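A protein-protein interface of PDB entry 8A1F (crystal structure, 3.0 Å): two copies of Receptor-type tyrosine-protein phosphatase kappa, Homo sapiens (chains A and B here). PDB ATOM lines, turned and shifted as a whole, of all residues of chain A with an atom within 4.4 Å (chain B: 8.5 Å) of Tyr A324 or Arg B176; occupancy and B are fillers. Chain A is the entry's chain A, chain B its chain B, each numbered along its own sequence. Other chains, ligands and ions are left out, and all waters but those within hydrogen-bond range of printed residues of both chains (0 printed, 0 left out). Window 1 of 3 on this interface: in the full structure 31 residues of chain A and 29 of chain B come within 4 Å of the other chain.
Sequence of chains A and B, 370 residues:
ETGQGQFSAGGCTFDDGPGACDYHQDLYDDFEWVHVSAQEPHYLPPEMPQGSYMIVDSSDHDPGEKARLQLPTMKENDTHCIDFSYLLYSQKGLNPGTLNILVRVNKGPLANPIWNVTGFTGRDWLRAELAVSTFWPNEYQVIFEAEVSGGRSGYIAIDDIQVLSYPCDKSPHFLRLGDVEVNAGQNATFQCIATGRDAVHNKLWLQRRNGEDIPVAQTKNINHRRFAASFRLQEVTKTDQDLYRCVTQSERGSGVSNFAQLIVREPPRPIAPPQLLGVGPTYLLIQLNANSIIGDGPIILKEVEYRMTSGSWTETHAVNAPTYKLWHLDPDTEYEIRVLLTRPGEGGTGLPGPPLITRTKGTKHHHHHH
Of the 11 printed residues of chain A, 5 touch a printed residue of chain B. Printed residues of chain A that touch a printed residue of chain B: Glu A315, His A317, Tyr A324, Lys A325 and Trp A327. Hydrophobic or aromatic side chains of chain A within 4 Å of the printed part of chain B: His A317, Tyr A324 and Trp A327. Of the 20 printed residues of chain B, 6 touch a printed residue of chain A. Printed residues of chain B that touch a printed residue of chain A: Phe B135, Trp B136, Leu B175, Arg B176, Ile B193 and Asn B258. Hydrophobic or aromatic side chains of chain B that line the printed part of chain A: Phe B135, Leu B175 and Ile B193. Among the printed residues, no Asp or Glu carboxylate lies within 4 Å of a Lys or Arg side-chain nitrogen of the other chain.
The backbone carbonyl oxygen (O) of Tyr A324 lies within hydrogen-bond range of the backbone NH (N) of Ile A286. The side-chain carboxylate (OE2) of Glu A315 sits at hydrogen-bond distance from a ring nitrogen (NE2) of His A317, 3.0 Å away. ND1 of His A317 sits at hydrogen-bond distance from OH of Tyr A324, at 2.8 Å. N of Leu B175 lies within hydrogen-bond range of O of Ile B193, 2.9 Å away. The backbone carbonyl oxygen of Leu B177 sits at hydrogen-bond distance from the side-chain amide nitrogen of Asn B258 (2.8 Å).
OE2 of Glu A315 touches CG1 of Ile B193, at 3.7 Å. CG of Trp A327 touches CE2 of Phe B135, 3.3 Å away. Leu B175 touches Trp A327 (CD2 to O, 3.6 Å). Arg B176 touches Trp A327 (CA to NE1, 3.4 Å). Trp A327 touches Asn B258 (CZ2 to CG, 3.7 Å).
The backbone carbonyl oxygen (O) of Arg B176 lies close to a ring nitrogen (NE2) of His A317 (3.4 Å). OH of Tyr A324 lies close to NE of Arg B176, 3.5 Å away. O of Trp B136 sits at hydrogen-bond distance from NZ of Lys A325, 3.1 Å away. O of Lys A325 sits at hydrogen-bond distance from NH1 of Arg B176 (2.8 Å).
No position is printed for both chains. Of the 9 pairs that touch across the chains among the printed residues, none has its exchanged pair printed and touching as well.
Tyr A324 touches one residue of chain B. Of chain A, only His A317 (3.1 Å), Tyr A324 (3.4 Å), Lys A325 (2.8 Å) and Trp A327 (3.4 Å) come within 4 Å of Arg B176. Thr A323 touches none of the printed residues of chain B. Printed residues of chain A within 4 Å of Leu B175: Trp A327 (3.6 Å). Of the printed residues of chain A, Trp B136 touches Lys A325 (3.1 Å). Printed residues of chain B within 4 Å of His A317: Arg B176 (3.1 Å). Of the printed residues of chain B, Trp A327 touches Phe B135, Leu B175, Arg B176 and Asn B258. Of the printed residues of chain B, Glu A315 touches Ile B193 (3.7 Å). His B173 touches none of the printed residues of chain A. The nearest residue of chain A that does not touch Arg B176 is Glu A315 (4.2 Å).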
ATOM      1  N   LEU A 284      25.932  10.007  34.065  1.00  0.00           N
ATOM      2  CA  LEU A 284      25.991   8.637  34.558  1.00  0.00           C
ATOM      3  C   LEU A 284      25.760   7.692  33.389  1.00  0.00           C
ATOM      4  O   LEU A 284      24.803   7.866  32.628  1.00  0.00           O
ATOM      5  CB  LEU A 284      24.934   8.386  35.644  1.00  0.00           C
ATOM      6  CG  LEU A 284      25.034   9.093  36.996  1.00  0.00           C
ATOM      7  CD1 LEU A 284      23.713   8.971  37.744  1.00  0.00           C
ATOM      8  CD2 LEU A 284      26.161   8.504  37.818  1.00  0.00           C
ATOM      9  N   LEU A 285      26.631   6.696  33.248  1.00  0.00           N
ATOM     10  CA  LEU A 285      26.460   5.625  32.272  1.00  0.00           C
ATOM     11  C   LEU A 285      26.158   4.342  33.033  1.00  0.00           C
ATOM     12  O   LEU A 285      26.971   3.895  33.851  1.00  0.00           O
ATOM     13  CB  LEU A 285      27.706   5.470  31.399  1.00  0.00           C
ATOM     14  CG  LEU A 285      27.695   4.346  30.363  1.00  0.00           C
ATOM     15  CD1 LEU A 285      26.743   4.683  29.228  1.00  0.00           C
ATOM     16  CD2 LEU A 285      29.100   4.106  29.836  1.00  0.00           C
ATOM     17  N   ILE A 286      24.997   3.749  32.759  1.00  0.00           N
ATOM     18  CA  ILE A 286      24.422   2.722  33.616  1.00  0.00           C
ATOM     19  C   ILE A 286      24.122   1.470  32.803  1.00  0.00           C
ATOM     20  O   ILE A 286      23.636   1.552  31.669  1.00  0.00           O
ATOM     21  CB  ILE A 286      23.145   3.243  34.307  1.00  0.00           C
ATOM     22  CG1 ILE A 286      23.510   4.343  35.302  1.00  0.00           C
ATOM     23  CG2 ILE A 286      22.398   2.116  35.000  1.00  0.00           C
ATOM     24  CD1 ILE A 286      22.325   4.971  35.974  1.00  0.00           C
ATOM     25  N   GLU A 315      11.959  10.827  36.734  1.00  0.00           N
ATOM     26  CA  GLU A 315      11.950  10.860  35.275  1.00  0.00           C
ATOM     27  C   GLU A 315      11.968   9.434  34.739  1.00  0.00           C
ATOM     28  O   GLU A 315      12.837   8.641  35.113  1.00  0.00           O
ATOM     29  CB  GLU A 315      13.164  11.636  34.751  1.00  0.00           C
ATOM     30  CG  GLU A 315      13.231  11.833  33.238  1.00  0.00           C
ATOM     31  CD  GLU A 315      12.338  12.946  32.728  1.00  0.00           C
ATOM     32  OE1 GLU A 315      11.467  13.423  33.486  1.00  0.00           O
ATOM     33  OE2 GLU A 315      12.519  13.354  31.560  1.00  0.00           O
ATOM     34  N   HIS A 317      11.869   6.860  31.359  1.00  0.00           N
ATOM     35  CA  HIS A 317      12.180   6.740  29.939  1.00  0.00           C
ATOM     36  C   HIS A 317      12.064   5.294  29.475  1.00  0.00           C
ATOM     37  O   HIS A 317      12.462   4.370  30.192  1.00  0.00           O
ATOM     38  CB  HIS A 317      13.591   7.247  29.635  1.00  0.00           C
ATOM     39  CG  HIS A 317      13.757   8.724  29.813  1.00  0.00           C
ATOM     40  ND1 HIS A 317      14.990   9.336  29.803  1.00  0.00           N
ATOM     41  CD2 HIS A 317      12.846   9.710  29.998  1.00  0.00           C
ATOM     42  CE1 HIS A 317      14.834  10.636  29.974  1.00  0.00           C
ATOM     43  NE2 HIS A 317      13.543  10.890  30.095  1.00  0.00           N
ATOM     44  N   VAL A 319      13.516   2.407  27.359  1.00  0.00           N
ATOM     45  CA  VAL A 319      14.872   2.069  26.943  1.00  0.00           C
ATOM     46  C   VAL A 319      14.881   0.647  26.399  1.00  0.00           C
ATOM     47  O   VAL A 319      14.305  -0.259  27.011  1.00  0.00           O
ATOM     48  CB  VAL A 319      15.876   2.204  28.105  1.00  0.00           C
ATOM     49  CG1 VAL A 319      17.287   1.859  27.637  1.00  0.00           C
ATOM     50  CG2 VAL A 319      15.829   3.609  28.691  1.00  0.00           C
ATOM     51  N   THR A 323      22.353  -0.656  28.089  1.00  0.00           N
ATOM     52  CA  THR A 323      22.953   0.464  28.795  1.00  0.00           C
ATOM     53  C   THR A 323      22.220   1.753  28.443  1.00  0.00           C
ATOM     54  O   THR A 323      21.660   1.893  27.352  1.00  0.00           O
ATOM     55  CB  THR A 323      24.443   0.601  28.465  1.00  0.00           C
ATOM     56  OG1 THR A 323      25.003   1.698  29.199  1.00  0.00           O
ATOM     57  CG2 THR A 323      24.636   0.832  26.978  1.00  0.00           C
ATOM     58  N   TYR A 324      22.212   2.684  29.396  1.00  0.00           N
ATOM     59  CA  TYR A 324      21.569   3.979  29.229  1.00  0.00           C
ATOM     60  C   TYR A 324      22.459   5.047  29.851  1.00  0.00           C
ATOM     61  O   TYR A 324      23.211   4.779  30.792  1.00  0.00           O
ATOM     62  CB  TYR A 324      20.167   3.980  29.867  1.00  0.00           C
ATOM     63  CG  TYR A 324      19.227   5.054  29.358  1.00  0.00           C
ATOM     64  CD1 TYR A 324      18.963   5.191  28.000  1.00  0.00           C
ATOM     65  CD2 TYR A 324      18.576   5.910  30.240  1.00  0.00           C
ATOM     66  CE1 TYR A 324      18.099   6.164  27.532  1.00  0.00           C
ATOM     67  CE2 TYR A 324      17.704   6.886  29.779  1.00  0.00           C
ATOM     68  CZ  TYR A 324      17.471   7.008  28.425  1.00  0.00           C
ATOM     69  OH  TYR A 324      16.607   7.975  27.962  1.00  0.00           O
ATOM     70  N   LYS A 325      22.370   6.261  29.315  1.00  0.00           N
ATOM     71  CA  LYS A 325      23.219   7.365  29.744  1.00  0.00           C
ATOM     72  C   LYS A 325      22.356   8.570  30.081  1.00  0.00           C
ATOM     73  O   LYS A 325      21.466   8.940  29.309  1.00  0.00           O
ATOM     74  CB  LYS A 325      24.239   7.719  28.655  1.00  0.00           C
ATOM     75  CG  LYS A 325      25.310   8.714  29.069  1.00  0.00           C
ATOM     76  CD  LYS A 325      26.321   8.915  27.942  1.00  0.00           C
ATOM     77  CE  LYS A 325      27.385   9.939  28.309  1.00  0.00           C
ATOM     78  NZ  LYS A 325      28.458   9.999  27.276  1.00  0.00           N
ATOM     79  N   LEU A 326      22.620   9.174  31.234  1.00  0.00           N
ATOM     80  CA  LEU A 326      21.902  10.346  31.711  1.00  0.00           C
ATOM     81  C   LEU A 326      22.870  11.518  31.763  1.00  0.00           C
ATOM     82  O   LEU A 326      24.033  11.342  32.131  1.00  0.00           O
ATOM     83  CB  LEU A 326      21.313  10.080  33.095  1.00  0.00           C
ATOM     84  CG  LEU A 326      20.480   8.801  33.200  1.00  0.00           C
ATOM     85  CD1 LEU A 326      20.014   8.555  34.630  1.00  0.00           C
ATOM     86  CD2 LEU A 326      19.293   8.848  32.252  1.00  0.00           C
ATOM     87  N   TRP A 327      22.402  12.713  31.399  1.00  0.00           N
ATOM     88  CA  TRP A 327      23.318  13.835  31.235  1.00  0.00           C
ATOM     89  C   TRP A 327      22.669  15.141  31.677  1.00  0.00           C
ATOM     90  O   TRP A 327      21.460  15.218  31.918  1.00  0.00           O
ATOM     91  CB  TRP A 327      23.849  13.922  29.796  1.00  0.00           C
ATOM     92  CG  TRP A 327      22.822  13.855  28.697  1.00  0.00           C
ATOM     93  CD1 TRP A 327      21.760  14.693  28.496  1.00  0.00           C
ATOM     94  CD2 TRP A 327      22.801  12.915  27.617  1.00  0.00           C
ATOM     95  NE1 TRP A 327      21.067  14.311  27.368  1.00  0.00           N
ATOM     96  CE2 TRP A 327      21.689  13.224  26.812  1.00  0.00           C
ATOM     97  CE3 TRP A 327      23.615  11.835  27.259  1.00  0.00           C
ATOM     98  CZ2 TRP A 327      21.368  12.489  25.669  1.00  0.00           C
ATOM     99  CZ3 TRP A 327      23.297  11.109  26.126  1.00  0.00           C
ATOM    100  CH2 TRP A 327      22.185  11.439  25.345  1.00  0.00           C
ATOM    101  N   SER B 133      22.702  19.430  24.177  1.00  0.00           N
ATOM    102  CA  SER B 133      22.716  18.130  24.837  1.00  0.00           C
ATOM    103  C   SER B 133      22.958  16.987  23.856  1.00  0.00           C
ATOM    104  O   SER B 133      22.182  16.027  23.816  1.00  0.00           O
ATOM    105  CB  SER B 133      21.397  17.903  25.579  1.00  0.00           C
ATOM    106  OG  SER B 133      21.080  19.015  26.395  1.00  0.00           O
ATOM    107  N   PHE B 135      25.991  14.281  22.955  1.00  0.00           N
ATOM    108  CA  PHE B 135      27.194  13.780  23.600  1.00  0.00           C
ATOM    109  C   PHE B 135      27.656  12.489  22.942  1.00  0.00           C
ATOM    110  O   PHE B 135      26.903  11.824  22.228  1.00  0.00           O
ATOM    111  CB  PHE B 135      26.957  13.539  25.095  1.00  0.00           C
ATOM    112  CG  PHE B 135      26.498  14.758  25.840  1.00  0.00           C
ATOM    113  CD1 PHE B 135      27.353  15.829  26.038  1.00  0.00           C
ATOM    114  CD2 PHE B 135      25.204  14.842  26.322  1.00  0.00           C
ATOM    115  CE1 PHE B 135      26.928  16.956  26.719  1.00  0.00           C
ATOM    116  CE2 PHE B 135      24.773  15.965  27.002  1.00  0.00           C
ATOM    117  CZ  PHE B 135      25.636  17.022  27.202  1.00  0.00           C
ATOM    118  N   TRP B 136      28.920  12.157  23.186  1.00  0.00           N
ATOM    119  CA  TRP B 136      29.485  10.899  22.717  1.00  0.00           C
ATOM    120  C   TRP B 136      28.573   9.740  23.118  1.00  0.00           C
ATOM    121  O   TRP B 136      28.063   9.715  24.246  1.00  0.00           O
ATOM    122  CB  TRP B 136      30.887  10.708  23.305  1.00  0.00           C
ATOM    123  CG  TRP B 136      31.627   9.507  22.797  1.00  0.00           C
ATOM    124  CD1 TRP B 136      32.581   9.488  21.824  1.00  0.00           C
ATOM    125  CD2 TRP B 136      31.491   8.155  23.253  1.00  0.00           C
ATOM    126  NE1 TRP B 136      33.044   8.208  21.640  1.00  0.00           N
ATOM    127  CE2 TRP B 136      32.388   7.371  22.503  1.00  0.00           C
ATOM    128  CE3 TRP B 136      30.695   7.532  24.218  1.00  0.00           C
ATOM    129  CZ2 TRP B 136      32.511   5.997  22.688  1.00  0.00           C
ATOM    130  CZ3 TRP B 136      30.817   6.169  24.400  1.00  0.00           C
ATOM    131  CH2 TRP B 136      31.717   5.416  23.639  1.00  0.00           C
ATOM    132  N   PRO B 137      28.351   8.759  22.234  1.00  0.00           N
ATOM    133  CA  PRO B 137      28.985   8.543  20.923  1.00  0.00           C
ATOM    134  C   PRO B 137      28.409   9.402  19.800  1.00  0.00           C
ATOM    135  O   PRO B 137      28.803   9.261  18.643  1.00  0.00           O
ATOM    136  CB  PRO B 137      28.727   7.052  20.682  1.00  0.00           C
ATOM    137  CG  PRO B 137      27.385   6.830  21.318  1.00  0.00           C
ATOM    138  CD  PRO B 137      27.410   7.675  22.569  1.00  0.00           C
ATOM    139  N   ASN B 138      27.473  10.294  20.097  1.00  0.00           N
ATOM    140  CA  ASN B 138      26.931  11.195  19.092  1.00  0.00           C
ATOM    141  C   ASN B 138      27.761  12.474  19.027  1.00  0.00           C
ATOM    142  O   ASN B 138      28.479  12.828  19.966  1.00  0.00           O
ATOM    143  CB  ASN B 138      25.463  11.513  19.387  1.00  0.00           C
ATOM    144  CG  ASN B 138      24.586  10.272  19.377  1.00  0.00           C
ATOM    145  OD1 ASN B 138      24.425   9.617  18.347  1.00  0.00           O
ATOM    146  ND2 ASN B 138      24.020   9.941  20.530  1.00  0.00           N
ATOM    147  N   HIS B 173      19.562  24.230  30.077  1.00  0.00           N
ATOM    148  CA  HIS B 173      20.088  22.909  29.754  1.00  0.00           C
ATOM    149  C   HIS B 173      18.945  21.905  29.803  1.00  0.00           C
ATOM    150  O   HIS B 173      18.252  21.804  30.819  1.00  0.00           O
ATOM    151  CB  HIS B 173      21.185  22.484  30.735  1.00  0.00           C
ATOM    152  CG  HIS B 173      22.345  23.428  30.797  1.00  0.00           C
ATOM    153  ND1 HIS B 173      23.321  23.471  29.824  1.00  0.00           N
ATOM    154  CD2 HIS B 173      22.684  24.367  31.712  1.00  0.00           C
ATOM    155  CE1 HIS B 173      24.210  24.396  30.138  1.00  0.00           C
ATOM    156  NE2 HIS B 173      23.848  24.954  31.278  1.00  0.00           N
ATOM    157  N   PHE B 174      18.755  21.162  28.716  1.00  0.00           N
ATOM    158  CA  PHE B 174      17.749  20.107  28.674  1.00  0.00           C
ATOM    159  C   PHE B 174      18.332  18.787  29.168  1.00  0.00           C
ATOM    160  O   PHE B 174      19.419  18.383  28.741  1.00  0.00           O
ATOM    161  CB  PHE B 174      17.200  19.931  27.256  1.00  0.00           C
ATOM    162  CG  PHE B 174      16.271  21.028  26.824  1.00  0.00           C
ATOM    163  CD1 PHE B 174      15.016  21.154  27.392  1.00  0.00           C
ATOM    164  CD2 PHE B 174      16.646  21.920  25.832  1.00  0.00           C
ATOM    165  CE1 PHE B 174      14.157  22.158  26.995  1.00  0.00           C
ATOM    166  CE2 PHE B 174      15.788  22.924  25.426  1.00  0.00           C
ATOM    167  CZ  PHE B 174      14.542  23.044  26.009  1.00  0.00           C
ATOM    168  N   LEU B 175      17.604  18.114  30.058  1.00  0.00           N
ATOM    169  CA  LEU B 175      17.907  16.724  30.354  1.00  0.00           C
ATOM    170  C   LEU B 175      17.626  15.858  29.124  1.00  0.00           C
ATOM    171  O   LEU B 175      17.088  16.322  28.113  1.00  0.00           O
ATOM    172  CB  LEU B 175      17.094  16.238  31.558  1.00  0.00           C
ATOM    173  CG  LEU B 175      17.224  17.053  32.847  1.00  0.00           C
ATOM    174  CD1 LEU B 175      16.449  16.399  33.978  1.00  0.00           C
ATOM    175  CD2 LEU B 175      18.685  17.190  33.230  1.00  0.00           C
ATOM    176  N   ARG B 176      17.985  14.580  29.222  1.00  0.00           N
ATOM    177  CA  ARG B 176      17.791  13.670  28.101  1.00  0.00           C
ATOM    178  C   ARG B 176      16.320  13.552  27.721  1.00  0.00           C
ATOM    179  O   ARG B 176      15.459  13.287  28.566  1.00  0.00           O
ATOM    180  CB  ARG B 176      18.356  12.285  28.421  1.00  0.00           C
ATOM    181  CG  ARG B 176      18.292  11.359  27.219  1.00  0.00           C
ATOM    182  CD  ARG B 176      19.165  10.132  27.356  1.00  0.00           C
ATOM    183  NE  ARG B 176      19.187   9.365  26.115  1.00  0.00           N
ATOM    184  CZ  ARG B 176      20.124   8.486  25.787  1.00  0.00           C
ATOM    185  NH1 ARG B 176      21.112   8.188  26.615  1.00  0.00           N
ATOM    186  NH2 ARG B 176      20.053   7.873  24.608  1.00  0.00           N
ATOM    187  N   LEU B 177      16.044  13.752  26.435  1.00  0.00           N
ATOM    188  CA  LEU B 177      14.723  13.515  25.870  1.00  0.00           C
ATOM    189  C   LEU B 177      14.642  12.064  25.405  1.00  0.00           C
ATOM    190  O   LEU B 177      15.455  11.620  24.588  1.00  0.00           O
ATOM    191  CB  LEU B 177      14.456  14.482  24.715  1.00  0.00           C
ATOM    192  CG  LEU B 177      13.086  14.451  24.038  1.00  0.00           C
ATOM    193  CD1 LEU B 177      11.992  14.815  25.021  1.00  0.00           C
ATOM    194  CD2 LEU B 177      13.071  15.389  22.840  1.00  0.00           C
ATOM    195  N   GLY B 178      13.658  11.333  25.923  1.00  0.00           N
ATOM    196  CA  GLY B 178      13.523   9.928  25.592  1.00  0.00           C
ATOM    197  C   GLY B 178      12.837   9.703  24.258  1.00  0.00           C
ATOM    198  O   GLY B 178      11.979  10.474  23.829  1.00  0.00           O
ATOM    199  N   ASP B 179      13.232   8.621  23.593  1.00  0.00           N
ATOM    200  CA  ASP B 179      12.540   8.198  22.382  1.00  0.00           C
ATOM    201  C   ASP B 179      11.090   7.842  22.696  1.00  0.00           C
ATOM    202  O   ASP B 179      10.754   7.432  23.812  1.00  0.00           O
ATOM    203  CB  ASP B 179      13.259   7.002  21.752  1.00  0.00           C
ATOM    204  CG  ASP B 179      14.677   7.330  21.333  1.00  0.00           C
ATOM    205  OD1 ASP B 179      14.978   8.525  21.129  1.00  0.00           O
ATOM    206  OD2 ASP B 179      15.490   6.391  21.205  1.00  0.00           O
ATOM    207  N   GLN B 191       8.092  15.228  26.141  1.00  0.00           N
ATOM    208  CA  GLN B 191       8.222  16.049  27.344  1.00  0.00           C
ATOM    209  C   GLN B 191       9.687  16.387  27.594  1.00  0.00           C
ATOM    210  O   GLN B 191      10.523  15.485  27.715  1.00  0.00           O
ATOM    211  CB  GLN B 191       7.632  15.355  28.574  1.00  0.00           C
ATOM    212  CG  GLN B 191       7.862  16.151  29.848  1.00  0.00           C
ATOM    213  CD  GLN B 191       6.643  16.216  30.742  1.00  0.00           C
ATOM    214  OE1 GLN B 191       5.729  17.006  30.510  1.00  0.00           O
ATOM    215  NE2 GLN B 191       6.625  15.383  31.776  1.00  0.00           N
ATOM    216  N   CYS B 192       9.987  17.678  27.696  1.00  0.00           N
ATOM    217  CA  CYS B 192      11.345  18.161  27.910  1.00  0.00           C
ATOM    218  C   CYS B 192      11.486  18.801  29.286  1.00  0.00           C
ATOM    219  O   CYS B 192      10.600  19.534  29.734  1.00  0.00           O
ATOM    220  CB  CYS B 192      11.733  19.163  26.826  1.00  0.00           C
ATOM    221  SG  CYS B 192      12.066  18.365  25.252  1.00  0.00           S
ATOM    222  N   ILE B 193      12.607  18.521  29.952  1.00  0.00           N
ATOM    223  CA  ILE B 193      12.928  19.082  31.260  1.00  0.00           C
ATOM    224  C   ILE B 193      14.155  19.970  31.104  1.00  0.00           C
ATOM    225  O   ILE B 193      15.175  19.534  30.560  1.00  0.00           O
ATOM    226  CB  ILE B 193      13.180  17.976  32.302  1.00  0.00           C
ATOM    227  CG1 ILE B 193      12.070  16.924  32.247  1.00  0.00           C
ATOM    228  CG2 ILE B 193      13.299  18.569  33.695  1.00  0.00           C
ATOM    229  CD1 ILE B 193      10.705  17.454  32.594  1.00  0.00           C
ATOM    230  N   ALA B 194      14.057  21.211  31.586  1.00  0.00           N
ATOM    231  CA  ALA B 194      15.124  22.191  31.432  1.00  0.00           C
ATOM    232  C   ALA B 194      15.409  22.916  32.743  1.00  0.00           C
ATOM    233  O   ALA B 194      14.493  23.218  33.514  1.00  0.00           O
ATOM    234  CB  ALA B 194      14.789  23.226  30.356  1.00  0.00           C
ATOM    235  N   SER B 257      18.301  20.172  23.003  1.00  0.00           N
ATOM    236  CA  SER B 257      18.288  18.837  23.581  1.00  0.00           C
ATOM    237  C   SER B 257      18.868  17.825  22.595  1.00  0.00           C
ATOM    238  O   SER B 257      19.394  18.178  21.536  1.00  0.00           O
ATOM    239  CB  SER B 257      16.867  18.454  23.990  1.00  0.00           C
ATOM    240  OG  SER B 257      16.146  17.918  22.893  1.00  0.00           O
ATOM    241  N   ASN B 258      18.765  16.547  22.937  1.00  0.00           N
ATOM    242  CA  ASN B 258      19.183  15.486  22.038  1.00  0.00           C
ATOM    243  C   ASN B 258      18.064  15.161  21.056  1.00  0.00           C
ATOM    244  O   ASN B 258      16.879  15.367  21.338  1.00  0.00           O
ATOM    245  CB  ASN B 258      19.563  14.228  22.817  1.00  0.00           C
ATOM    246  CG  ASN B 258      18.476  13.802  23.789  1.00  0.00           C
ATOM    247  OD1 ASN B 258      18.234  14.460  24.801  1.00  0.00           O
ATOM    248  ND2 ASN B 258      17.792  12.705  23.466  1.00  0.00           N
ATOM    249  N   PHE B 259      18.448  14.664  19.887  1.00  0.00           N
ATOM    250  CA  PHE B 259      17.468  14.233  18.895  1.00  0.00           C
ATOM    251  C   PHE B 259      16.841  12.922  19.354  1.00  0.00           C
ATOM    252  O   PHE B 259      17.427  11.849  19.195  1.00  0.00           O
ATOM    253  CB  PHE B 259      18.123  14.090  17.526  1.00  0.00           C
ATOM    254  CG  PHE B 259      17.916  15.280  16.632  1.00  0.00           C
ATOM    255  CD1 PHE B 259      16.670  15.877  16.538  1.00  0.00           C
ATOM    256  CD2 PHE B 259      18.964  15.806  15.893  1.00  0.00           C
ATOM    257  CE1 PHE B 259      16.470  16.972  15.722  1.00  0.00           C
ATOM    258  CE2 PHE B 259      18.768  16.904  15.075  1.00  0.00           C
ATOM    259  CZ  PHE B 259      17.518  17.487  14.990  1.00  0.00           C
ATOM    260  N   ALA B 260      15.649  13.010  19.939  1.00  0.00           N
ATOM    261  CA  ALA B 260      14.880  11.827  20.295  1.00  0.00           C
ATOM    262  C   ALA B 260      14.099  11.326  19.087  1.00  0.00           C
ATOM    263  O   ALA B 260      13.737  12.095  18.191  1.00  0.00           O
ATOM    264  CB  ALA B 260      13.922  12.129  21.449  1.00  0.00           C
